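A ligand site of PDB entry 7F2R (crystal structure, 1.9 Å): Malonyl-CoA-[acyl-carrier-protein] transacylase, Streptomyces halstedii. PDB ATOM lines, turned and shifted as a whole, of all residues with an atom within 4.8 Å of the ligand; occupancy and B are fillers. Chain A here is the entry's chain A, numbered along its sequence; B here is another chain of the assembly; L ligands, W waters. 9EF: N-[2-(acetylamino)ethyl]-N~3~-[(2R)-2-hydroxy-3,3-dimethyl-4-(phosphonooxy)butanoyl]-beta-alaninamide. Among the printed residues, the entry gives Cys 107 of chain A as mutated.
OAG of the ligand is in salt-bridge range of NH1 of Arg 33 of chain B, at 3.4 Å. The side-chain sulfur (SG) of Cys 107 is covalently linked to a carbon (CAA) of the ligand (1.8 Å). An oxygen (OAD) of the ligand sits at hydrogen-bond distance from the side-chain sulfur (SG) of Cys 178 (3.2 Å). OG of Ser 39 of chain B is covalently linked to PAW of the ligand. N of Ser 39 of chain B is in hydrogen-bond range of OAG of the ligand (2.7 Å). A ring nitrogen (NE2) of His 217 is in hydrogen-bond range of an oxygen (OAD) of the ligand, 2.7 Å away.
O of Thr 149 is in hydrogen-bond range of N of Met 212, at 2.7 Å. The side-chain hydroxyl (OH) of Tyr 73 sits at hydrogen-bond distance from the backbone carbonyl oxygen (O) of Met 29 (2.8 Å). N of Leu 209 lies within hydrogen-bond range of O of Ser 151, at 2.9 Å. The backbone NH (N) of Met 216 lies within hydrogen-bond range of the side-chain hydroxyl (OG1) of Thr 149 (3.2 Å). N of Met 186 is in hydrogen-bond range of O of Cys 178 (3.1 Å). The backbone carbonyl oxygen (O) of Tyr 210 sits at hydrogen-bond distance from the backbone NH (N) of Ser 151. SG of Cys 107 lies within hydrogen-bond range of NE2 of His 217 (3.4 Å).
Met 29 touches the ligand (O to CAM, 3.6 Å). CD of Pro 31 touches OAF of the ligand, 3.7 Å away. Tyr 73 touches the ligand (OH to CAM, 2.9 Å). OG of Ser 151 touches CAB of the ligand, 3.3 Å away. Met 186 touches the ligand. CD2 of Tyr 210 touches OAE of the ligand (3.7 Å). CB of Met 212 touches OAE of the ligand (3.7 Å). Met 216 touches the ligand (SD to CAK, 3.98 Å). Leu 272 touches the ligand (CD2 to CAA, 3.8 Å). Leu 297 touches the ligand (CD2 to OAI, 3.3 Å). Asp 38 of chain B touches the ligand. Hydrophobic or aromatic side chains that line the ligand: Pro 31, Met 186, Tyr 210, Met 212, Met 216, His 217, Leu 272 and Leu 297.
Water W1 lies within hydrogen-bond range of an oxygen (OAG) of the ligand and the side-chain hydroxyl of Ser 296.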
ATOM      1  N   GLY A  28     -12.874  15.361  15.765  1.00  0.00           N
ATOM      2  CA  GLY A  28     -13.893  16.377  16.002  1.00  0.00           C
ATOM      3  C   GLY A  28     -14.876  16.391  14.830  1.00  0.00           C
ATOM      4  O   GLY A  28     -14.490  15.876  13.781  1.00  0.00           O
ATOM      5  N   MET A  29     -16.057  16.955  14.997  1.00  0.00           N
ATOM      6  CA  MET A  29     -17.060  17.005  13.881  1.00  0.00           C
ATOM      7  C   MET A  29     -16.861  18.281  13.057  1.00  0.00           C
ATOM      8  O   MET A  29     -16.919  19.403  13.616  1.00  0.00           O
ATOM      9  CB  MET A  29     -18.470  16.954  14.457  1.00  0.00           C
ATOM     10  CG  MET A  29     -19.561  16.875  13.365  1.00  0.00           C
ATOM     11  SD  MET A  29     -21.117  16.897  14.241  1.00  0.00           S
ATOM     12  CE  MET A  29     -22.263  17.010  12.858  1.00  0.00           C
ATOM     13  N   GLY A  30     -16.519  18.110  11.775  1.00  0.00           N
ATOM     14  CA  GLY A  30     -16.535  19.239  10.835  1.00  0.00           C
ATOM     15  C   GLY A  30     -17.914  19.386  10.198  1.00  0.00           C
ATOM     16  O   GLY A  30     -18.825  18.649  10.494  1.00  0.00           O
ATOM     17  N   PRO A  31     -18.117  20.429   9.401  1.00  0.00           N
ATOM     18  CA  PRO A  31     -19.421  20.691   8.797  1.00  0.00           C
ATOM     19  C   PRO A  31     -20.045  19.512   8.028  1.00  0.00           C
ATOM     20  O   PRO A  31     -19.492  19.129   7.059  1.00  0.00           O
ATOM     21  CB  PRO A  31     -19.041  21.870   7.896  1.00  0.00           C
ATOM     22  CG  PRO A  31     -17.963  22.568   8.675  1.00  0.00           C
ATOM     23  CD  PRO A  31     -17.074  21.423   9.071  1.00  0.00           C
ATOM     24  N   TYR A  73     -24.614  21.272  11.718  1.00  0.00           N
ATOM     25  CA  TYR A  73     -24.414  20.679  13.058  1.00  0.00           C
ATOM     26  C   TYR A  73     -25.755  20.351  13.673  1.00  0.00           C
ATOM     27  O   TYR A  73     -25.863  20.499  14.883  1.00  0.00           O
ATOM     28  CB  TYR A  73     -23.649  21.670  13.921  1.00  0.00           C
ATOM     29  CG  TYR A  73     -22.220  21.776  13.472  1.00  0.00           C
ATOM     30  CD1 TYR A  73     -21.381  20.752  13.825  1.00  0.00           C
ATOM     31  CD2 TYR A  73     -21.718  22.826  12.730  1.00  0.00           C
ATOM     32  CE1 TYR A  73     -20.063  20.753  13.476  1.00  0.00           C
ATOM     33  CE2 TYR A  73     -20.381  22.853  12.358  1.00  0.00           C
ATOM     34  CZ  TYR A  73     -19.540  21.807  12.755  1.00  0.00           C
ATOM     35  OH  TYR A  73     -18.195  21.698  12.527  1.00  0.00           O
ATOM     36  N   CYS A 107     -12.866  16.237  21.000  1.00  0.00           N
ATOM     37  CA  CYS A 107     -14.138  17.004  21.064  1.00  0.00           C
ATOM     38  C   CYS A 107     -15.289  15.999  20.852  1.00  0.00           C
ATOM     39  O   CYS A 107     -15.412  15.046  21.671  1.00  0.00           O
ATOM     40  CB  CYS A 107     -14.142  18.152  20.052  1.00  0.00           C
ATOM     41  SG  CYS A 107     -12.665  19.216  20.187  1.00  0.00           S
ATOM     42  N   THR A 149     -16.411  30.602  18.508  1.00  0.00           N
ATOM     43  CA  THR A 149     -15.076  29.943  18.632  1.00  0.00           C
ATOM     44  C   THR A 149     -14.376  30.090  17.280  1.00  0.00           C
ATOM     45  O   THR A 149     -14.855  29.495  16.304  1.00  0.00           O
ATOM     46  CB  THR A 149     -15.180  28.486  19.114  1.00  0.00           C
ATOM     47  OG1 THR A 149     -15.906  28.471  20.353  1.00  0.00           O
ATOM     48  CG2 THR A 149     -13.819  27.826  19.225  1.00  0.00           C
ATOM     49  N   SER A 151     -11.215  29.455  14.782  1.00  0.00           N
ATOM     50  CA  SER A 151      -9.993  28.658  14.476  1.00  0.00           C
ATOM     51  C   SER A 151      -9.095  29.520  13.562  1.00  0.00           C
ATOM     52  O   SER A 151      -9.643  30.192  12.720  1.00  0.00           O
ATOM     53  CB  SER A 151     -10.321  27.305  13.858  1.00  0.00           C
ATOM     54  OG  SER A 151     -11.353  27.440  12.897  1.00  0.00           O
ATOM     55  N   CYS A 178      -8.961  25.541  22.135  1.00  0.00           N
ATOM     56  CA  CYS A 178      -8.182  24.389  21.622  1.00  0.00           C
ATOM     57  C   CYS A 178      -6.729  24.799  21.391  1.00  0.00           C
ATOM     58  O   CYS A 178      -6.469  25.910  20.791  1.00  0.00           O
ATOM     59  CB  CYS A 178      -8.674  23.855  20.280  1.00  0.00           C
ATOM     60  SG  CYS A 178     -10.463  23.659  20.151  1.00  0.00           S
ATOM     61  N   PHE A 184      -1.513  26.723  15.755  1.00  0.00           N
ATOM     62  CA  PHE A 184      -2.950  26.469  15.375  1.00  0.00           C
ATOM     63  C   PHE A 184      -3.802  26.407  16.663  1.00  0.00           C
ATOM     64  O   PHE A 184      -3.579  25.498  17.487  1.00  0.00           O
ATOM     65  CB  PHE A 184      -2.963  25.189  14.534  1.00  0.00           C
ATOM     66  CG  PHE A 184      -4.243  24.810  13.839  1.00  0.00           C
ATOM     67  CD1 PHE A 184      -5.483  25.302  14.218  1.00  0.00           C
ATOM     68  CD2 PHE A 184      -4.183  23.929  12.767  1.00  0.00           C
ATOM     69  CE1 PHE A 184      -6.630  24.941  13.517  1.00  0.00           C
ATOM     70  CE2 PHE A 184      -5.335  23.561  12.071  1.00  0.00           C
ATOM     71  CZ  PHE A 184      -6.548  24.050  12.468  1.00  0.00           C
ATOM     72  N   MET A 186      -7.810  27.628  18.642  1.00  0.00           N
ATOM     73  CA  MET A 186      -9.196  28.140  18.653  1.00  0.00           C
ATOM     74  C   MET A 186      -9.326  29.108  19.848  1.00  0.00           C
ATOM     75  O   MET A 186      -8.733  28.828  20.971  1.00  0.00           O
ATOM     76  CB  MET A 186     -10.230  27.016  18.729  1.00  0.00           C
ATOM     77  CG  MET A 186     -10.469  26.302  17.411  1.00  0.00           C
ATOM     78  SD  MET A 186      -9.089  25.344  16.838  1.00  0.00           S
ATOM     79  CE  MET A 186     -10.026  24.198  15.832  1.00  0.00           C
ATOM     80  N   LEU A 209      -9.692  30.662   9.896  1.00  0.00           N
ATOM     81  CA  LEU A 209     -10.324  29.543   9.152  1.00  0.00           C
ATOM     82  C   LEU A 209     -11.830  29.608   9.320  1.00  0.00           C
ATOM     83  O   LEU A 209     -12.493  29.597   8.277  1.00  0.00           O
ATOM     84  CB  LEU A 209      -9.760  28.196   9.621  1.00  0.00           C
ATOM     85  CG  LEU A 209      -8.273  27.978   9.387  1.00  0.00           C
ATOM     86  CD1 LEU A 209      -7.863  26.591   9.874  1.00  0.00           C
ATOM     87  CD2 LEU A 209      -7.897  28.145   7.912  1.00  0.00           C
ATOM     88  N   TYR A 210     -12.353  29.572  10.548  1.00  0.00           N
ATOM     89  CA  TYR A 210     -13.799  29.338  10.810  1.00  0.00           C
ATOM     90  C   TYR A 210     -14.151  29.990  12.154  1.00  0.00           C
ATOM     91  O   TYR A 210     -13.278  30.104  13.057  1.00  0.00           O
ATOM     92  CB  TYR A 210     -14.106  27.844  10.748  1.00  0.00           C
ATOM     93  CG  TYR A 210     -15.540  27.355  10.721  1.00  0.00           C
ATOM     94  CD1 TYR A 210     -16.261  27.284   9.533  1.00  0.00           C
ATOM     95  CD2 TYR A 210     -16.123  26.794  11.849  1.00  0.00           C
ATOM     96  CE1 TYR A 210     -17.545  26.749   9.493  1.00  0.00           C
ATOM     97  CE2 TYR A 210     -17.417  26.297  11.826  1.00  0.00           C
ATOM     98  CZ  TYR A 210     -18.132  26.269  10.639  1.00  0.00           C
ATOM     99  OH  TYR A 210     -19.411  25.774  10.630  1.00  0.00           O
ATOM    100  N   MET A 212     -17.112  29.304  14.853  1.00  0.00           N
ATOM    101  CA  MET A 212     -18.077  28.205  15.182  1.00  0.00           C
ATOM    102  C   MET A 212     -19.139  28.794  16.133  1.00  0.00           C
ATOM    103  O   MET A 212     -18.776  29.504  17.089  1.00  0.00           O
ATOM    104  CB  MET A 212     -17.288  27.018  15.754  1.00  0.00           C
ATOM    105  CG  MET A 212     -18.100  25.778  16.256  1.00  0.00           C
ATOM    106  SD  MET A 212     -18.930  24.850  14.951  1.00  0.00           S
ATOM    107  CE  MET A 212     -19.988  23.759  15.907  1.00  0.00           C
ATOM    108  N   MET A 216     -17.508  26.323  22.009  1.00  0.00           N
ATOM    109  CA  MET A 216     -17.151  25.114  22.799  1.00  0.00           C
ATOM    110  C   MET A 216     -15.918  25.409  23.669  1.00  0.00           C
ATOM    111  O   MET A 216     -15.146  26.262  23.319  1.00  0.00           O
ATOM    112  CB  MET A 216     -16.802  23.942  21.864  1.00  0.00           C
ATOM    113  CG  MET A 216     -17.973  23.562  20.935  1.00  0.00           C
ATOM    114  SD  MET A 216     -17.425  22.540  19.494  1.00  0.00           S
ATOM    115  CE  MET A 216     -16.995  20.995  20.315  1.00  0.00           C
ATOM    116  N   HIS A 217     -15.847  24.770  24.819  1.00  0.00           N
ATOM    117  CA  HIS A 217     -14.658  24.615  25.700  1.00  0.00           C
ATOM    118  C   HIS A 217     -14.327  25.949  26.333  1.00  0.00           C
ATOM    119  O   HIS A 217     -13.471  26.644  25.760  1.00  0.00           O
ATOM    120  CB  HIS A 217     -13.391  24.163  24.947  1.00  0.00           C
ATOM    121  CG  HIS A 217     -13.577  23.032  23.993  1.00  0.00           C
ATOM    122  ND1 HIS A 217     -14.097  21.794  24.377  1.00  0.00           N
ATOM    123  CD2 HIS A 217     -13.320  22.972  22.662  1.00  0.00           C
ATOM    124  CE1 HIS A 217     -14.174  21.029  23.305  1.00  0.00           C
ATOM    125  NE2 HIS A 217     -13.655  21.717  22.231  1.00  0.00           N
ATOM    126  N   LEU A 272      -9.496  21.585  24.501  1.00  0.00           N
ATOM    127  CA  LEU A 272      -8.758  20.516  23.774  1.00  0.00           C
ATOM    128  C   LEU A 272      -7.274  20.828  23.799  1.00  0.00           C
ATOM    129  O   LEU A 272      -6.888  22.007  23.444  1.00  0.00           O
ATOM    130  CB  LEU A 272      -9.273  20.481  22.335  1.00  0.00           C
ATOM    131  CG  LEU A 272      -8.454  19.645  21.371  1.00  0.00           C
ATOM    132  CD1 LEU A 272      -8.431  18.208  21.809  1.00  0.00           C
ATOM    133  CD2 LEU A 272      -9.023  19.753  19.944  1.00  0.00           C
ATOM    134  N   SER A 296     -10.963  16.394   8.124  1.00  0.00           N
ATOM    135  CA  SER A 296      -9.903  17.125   7.401  1.00  0.00           C
ATOM    136  C   SER A 296      -9.120  18.010   8.365  1.00  0.00           C
ATOM    137  O   SER A 296      -8.501  18.972   7.877  1.00  0.00           O
ATOM    138  CB  SER A 296     -10.498  17.897   6.275  1.00  0.00           C
ATOM    139  OG  SER A 296     -11.500  18.707   6.858  1.00  0.00           O
ATOM    140  N   LEU A 297      -8.998  17.583   9.638  1.00  0.00           N
ATOM    141  CA  LEU A 297      -8.110  18.253  10.622  1.00  0.00           C
ATOM    142  C   LEU A 297      -7.181  17.260  11.319  1.00  0.00           C
ATOM    143  O   LEU A 297      -5.970  17.415  11.119  1.00  0.00           O
ATOM    144  CB  LEU A 297      -8.982  19.093  11.581  1.00  0.00           C
ATOM    145  CG  LEU A 297      -8.315  19.730  12.789  1.00  0.00           C
ATOM    146  CD1 LEU A 297      -7.033  20.494  12.435  1.00  0.00           C
ATOM    147  CD2 LEU A 297      -9.319  20.655  13.480  1.00  0.00           C
ATOM    148  N   PHE A 298      -7.688  16.275  12.111  1.00  0.00           N
ATOM    149  CA  PHE A 298      -6.883  15.433  13.043  1.00  0.00           C
ATOM    150  C   PHE A 298      -5.928  14.482  12.334  1.00  0.00           C
ATOM    151  O   PHE A 298      -4.754  14.319  12.822  1.00  0.00           O
ATOM    152  CB  PHE A 298      -7.835  14.767  14.044  1.00  0.00           C
ATOM    153  CG  PHE A 298      -8.427  15.858  14.880  1.00  0.00           C
ATOM    154  CD1 PHE A 298      -7.719  16.417  15.934  1.00  0.00           C
ATOM    155  CD2 PHE A 298      -9.625  16.465  14.504  1.00  0.00           C
ATOM    156  CE1 PHE A 298      -8.230  17.494  16.650  1.00  0.00           C
ATOM    157  CE2 PHE A 298     -10.157  17.530  15.242  1.00  0.00           C
ATOM    158  CZ  PHE A 298      -9.451  18.026  16.310  1.00  0.00           C
ATOM    159  N   ARG B  33     -12.163  25.351  -3.958  1.00  0.00           N
ATOM    160  CA  ARG B  33     -12.810  24.536  -2.890  1.00  0.00           C
ATOM    161  C   ARG B  33     -13.579  23.390  -3.538  1.00  0.00           C
ATOM    162  O   ARG B  33     -13.410  22.256  -3.072  1.00  0.00           O
ATOM    163  CB  ARG B  33     -13.727  25.388  -1.989  1.00  0.00           C
ATOM    164  CG  ARG B  33     -14.178  24.668  -0.707  1.00  0.00           C
ATOM    165  CD  ARG B  33     -14.615  25.524   0.486  1.00  0.00           C
ATOM    166  NE  ARG B  33     -13.483  26.149   1.197  1.00  0.00           N
ATOM    167  CZ  ARG B  33     -12.811  25.619   2.244  1.00  0.00           C
ATOM    168  NH1 ARG B  33     -13.158  24.459   2.770  1.00  0.00           N
ATOM    169  NH2 ARG B  33     -11.783  26.287   2.781  1.00  0.00           N
ATOM    170  N   ASP B  38      -8.964  22.822   0.486  1.00  0.00           N
ATOM    171  CA  ASP B  38      -9.631  22.937   1.814  1.00  0.00           C
ATOM    172  C   ASP B  38      -8.637  23.620   2.763  1.00  0.00           C
ATOM    173  O   ASP B  38      -7.663  24.165   2.257  1.00  0.00           O
ATOM    174  CB  ASP B  38     -10.108  21.569   2.278  1.00  0.00           C
ATOM    175  CG  ASP B  38      -9.002  20.565   2.548  1.00  0.00           C
ATOM    176  OD1 ASP B  38      -7.841  20.942   2.568  1.00  0.00           O
ATOM    177  OD2 ASP B  38      -9.327  19.424   2.808  1.00  0.00           O
ATOM    178  N   SER B  39      -8.940  23.689   4.066  1.00  0.00           N
ATOM    179  CA  SER B  39      -8.210  24.595   4.994  1.00  0.00           C
ATOM    180  C   SER B  39      -6.773  24.121   5.082  1.00  0.00           C
ATOM    181  O   SER B  39      -5.906  24.925   4.774  1.00  0.00           O
ATOM    182  CB  SER B  39      -8.834  24.712   6.377  1.00  0.00           C
ATOM    183  OG  SER B  39     -10.234  24.948   6.311  1.00  0.00           O
ATOM    184  N   LEU B  40      -6.550  22.840   5.364  1.00  0.00           N
ATOM    185  CA  LEU B  40      -5.162  22.369   5.585  1.00  0.00           C
ATOM    186  C   LEU B  40      -4.437  22.233   4.247  1.00  0.00           C
ATOM    187  O   LEU B  40      -3.232  22.407   4.232  1.00  0.00           O
ATOM    188  CB  LEU B  40      -5.221  21.090   6.401  1.00  0.00           C
ATOM    189  CG  LEU B  40      -5.409  21.318   7.887  1.00  0.00           C
ATOM    190  CD1 LEU B  40      -5.157  20.028   8.639  1.00  0.00           C
ATOM    191  CD2 LEU B  40      -4.462  22.381   8.402  1.00  0.00           C
HETATM  192  OAG 9EF L   1     -11.300  23.090   5.266  1.00  0.00           O
HETATM  193  PAW 9EF L   1     -11.642  24.100   6.266  1.00  0.00           P
HETATM  194  OAH 9EF L   1     -12.248  25.395   6.046  1.00  0.00           O
HETATM  195  OAR 9EF L   1     -11.533  23.444   7.835  1.00  0.00           O
HETATM  196  CAN 9EF L   1     -11.495  24.340   8.935  1.00  0.00           C
HETATM  197  CAX 9EF L   1     -11.243  23.511  10.211  1.00  0.00           C
HETATM  198  CAB 9EF L   1     -11.386  24.421  11.500  1.00  0.00           C
HETATM  199  CAC 9EF L   1      -9.834  22.902  10.111  1.00  0.00           C
HETATM  200  CAV 9EF L   1     -12.197  22.298  10.338  1.00  0.00           C
HETATM  201  OAI 9EF L   1     -11.770  21.642  11.523  1.00  0.00           O
HETATM  202  CAU 9EF L   1     -13.573  22.782  10.598  1.00  0.00           C
HETATM  203  OAF 9EF L   1     -14.128  23.476   9.758  1.00  0.00           O
HETATM  204  NAQ 9EF L   1     -13.990  22.697  11.859  1.00  0.00           N
HETATM  205  CAL 9EF L   1     -15.344  23.182  12.224  1.00  0.00           C
HETATM  206  CAM 9EF L   1     -15.705  22.781  13.657  1.00  0.00           C
HETATM  207  CAT 9EF L   1     -15.033  23.686  14.740  1.00  0.00           C
HETATM  208  OAE 9EF L   1     -14.609  24.791  14.503  1.00  0.00           O
HETATM  209  NAP 9EF L   1     -15.058  23.187  16.001  1.00  0.00           N
HETATM  210  CAK 9EF L   1     -14.529  23.939  17.154  1.00  0.00           C
HETATM  211  CAJ 9EF L   1     -13.044  23.674  17.241  1.00  0.00           C
HETATM  212  NAO 9EF L   1     -12.776  22.215  17.414  1.00  0.00           N
HETATM  213  CAS 9EF L   1     -12.896  21.612  18.618  1.00  0.00           C
HETATM  214  OAD 9EF L   1     -13.224  22.202  19.625  1.00  0.00           O
HETATM  215  CAA 9EF L   1     -12.589  20.095  18.623  1.00  0.00           C
HETATM  216  O   HOH W   1     -12.676  20.529   4.839  1.00  0.00           O
HETATM  217  O   HOH W   2     -13.240  19.729  15.270  1.00  0.00           O
HETATM  218  O   HOH W   3     -13.803  27.199  14.671  1.00  0.00           O
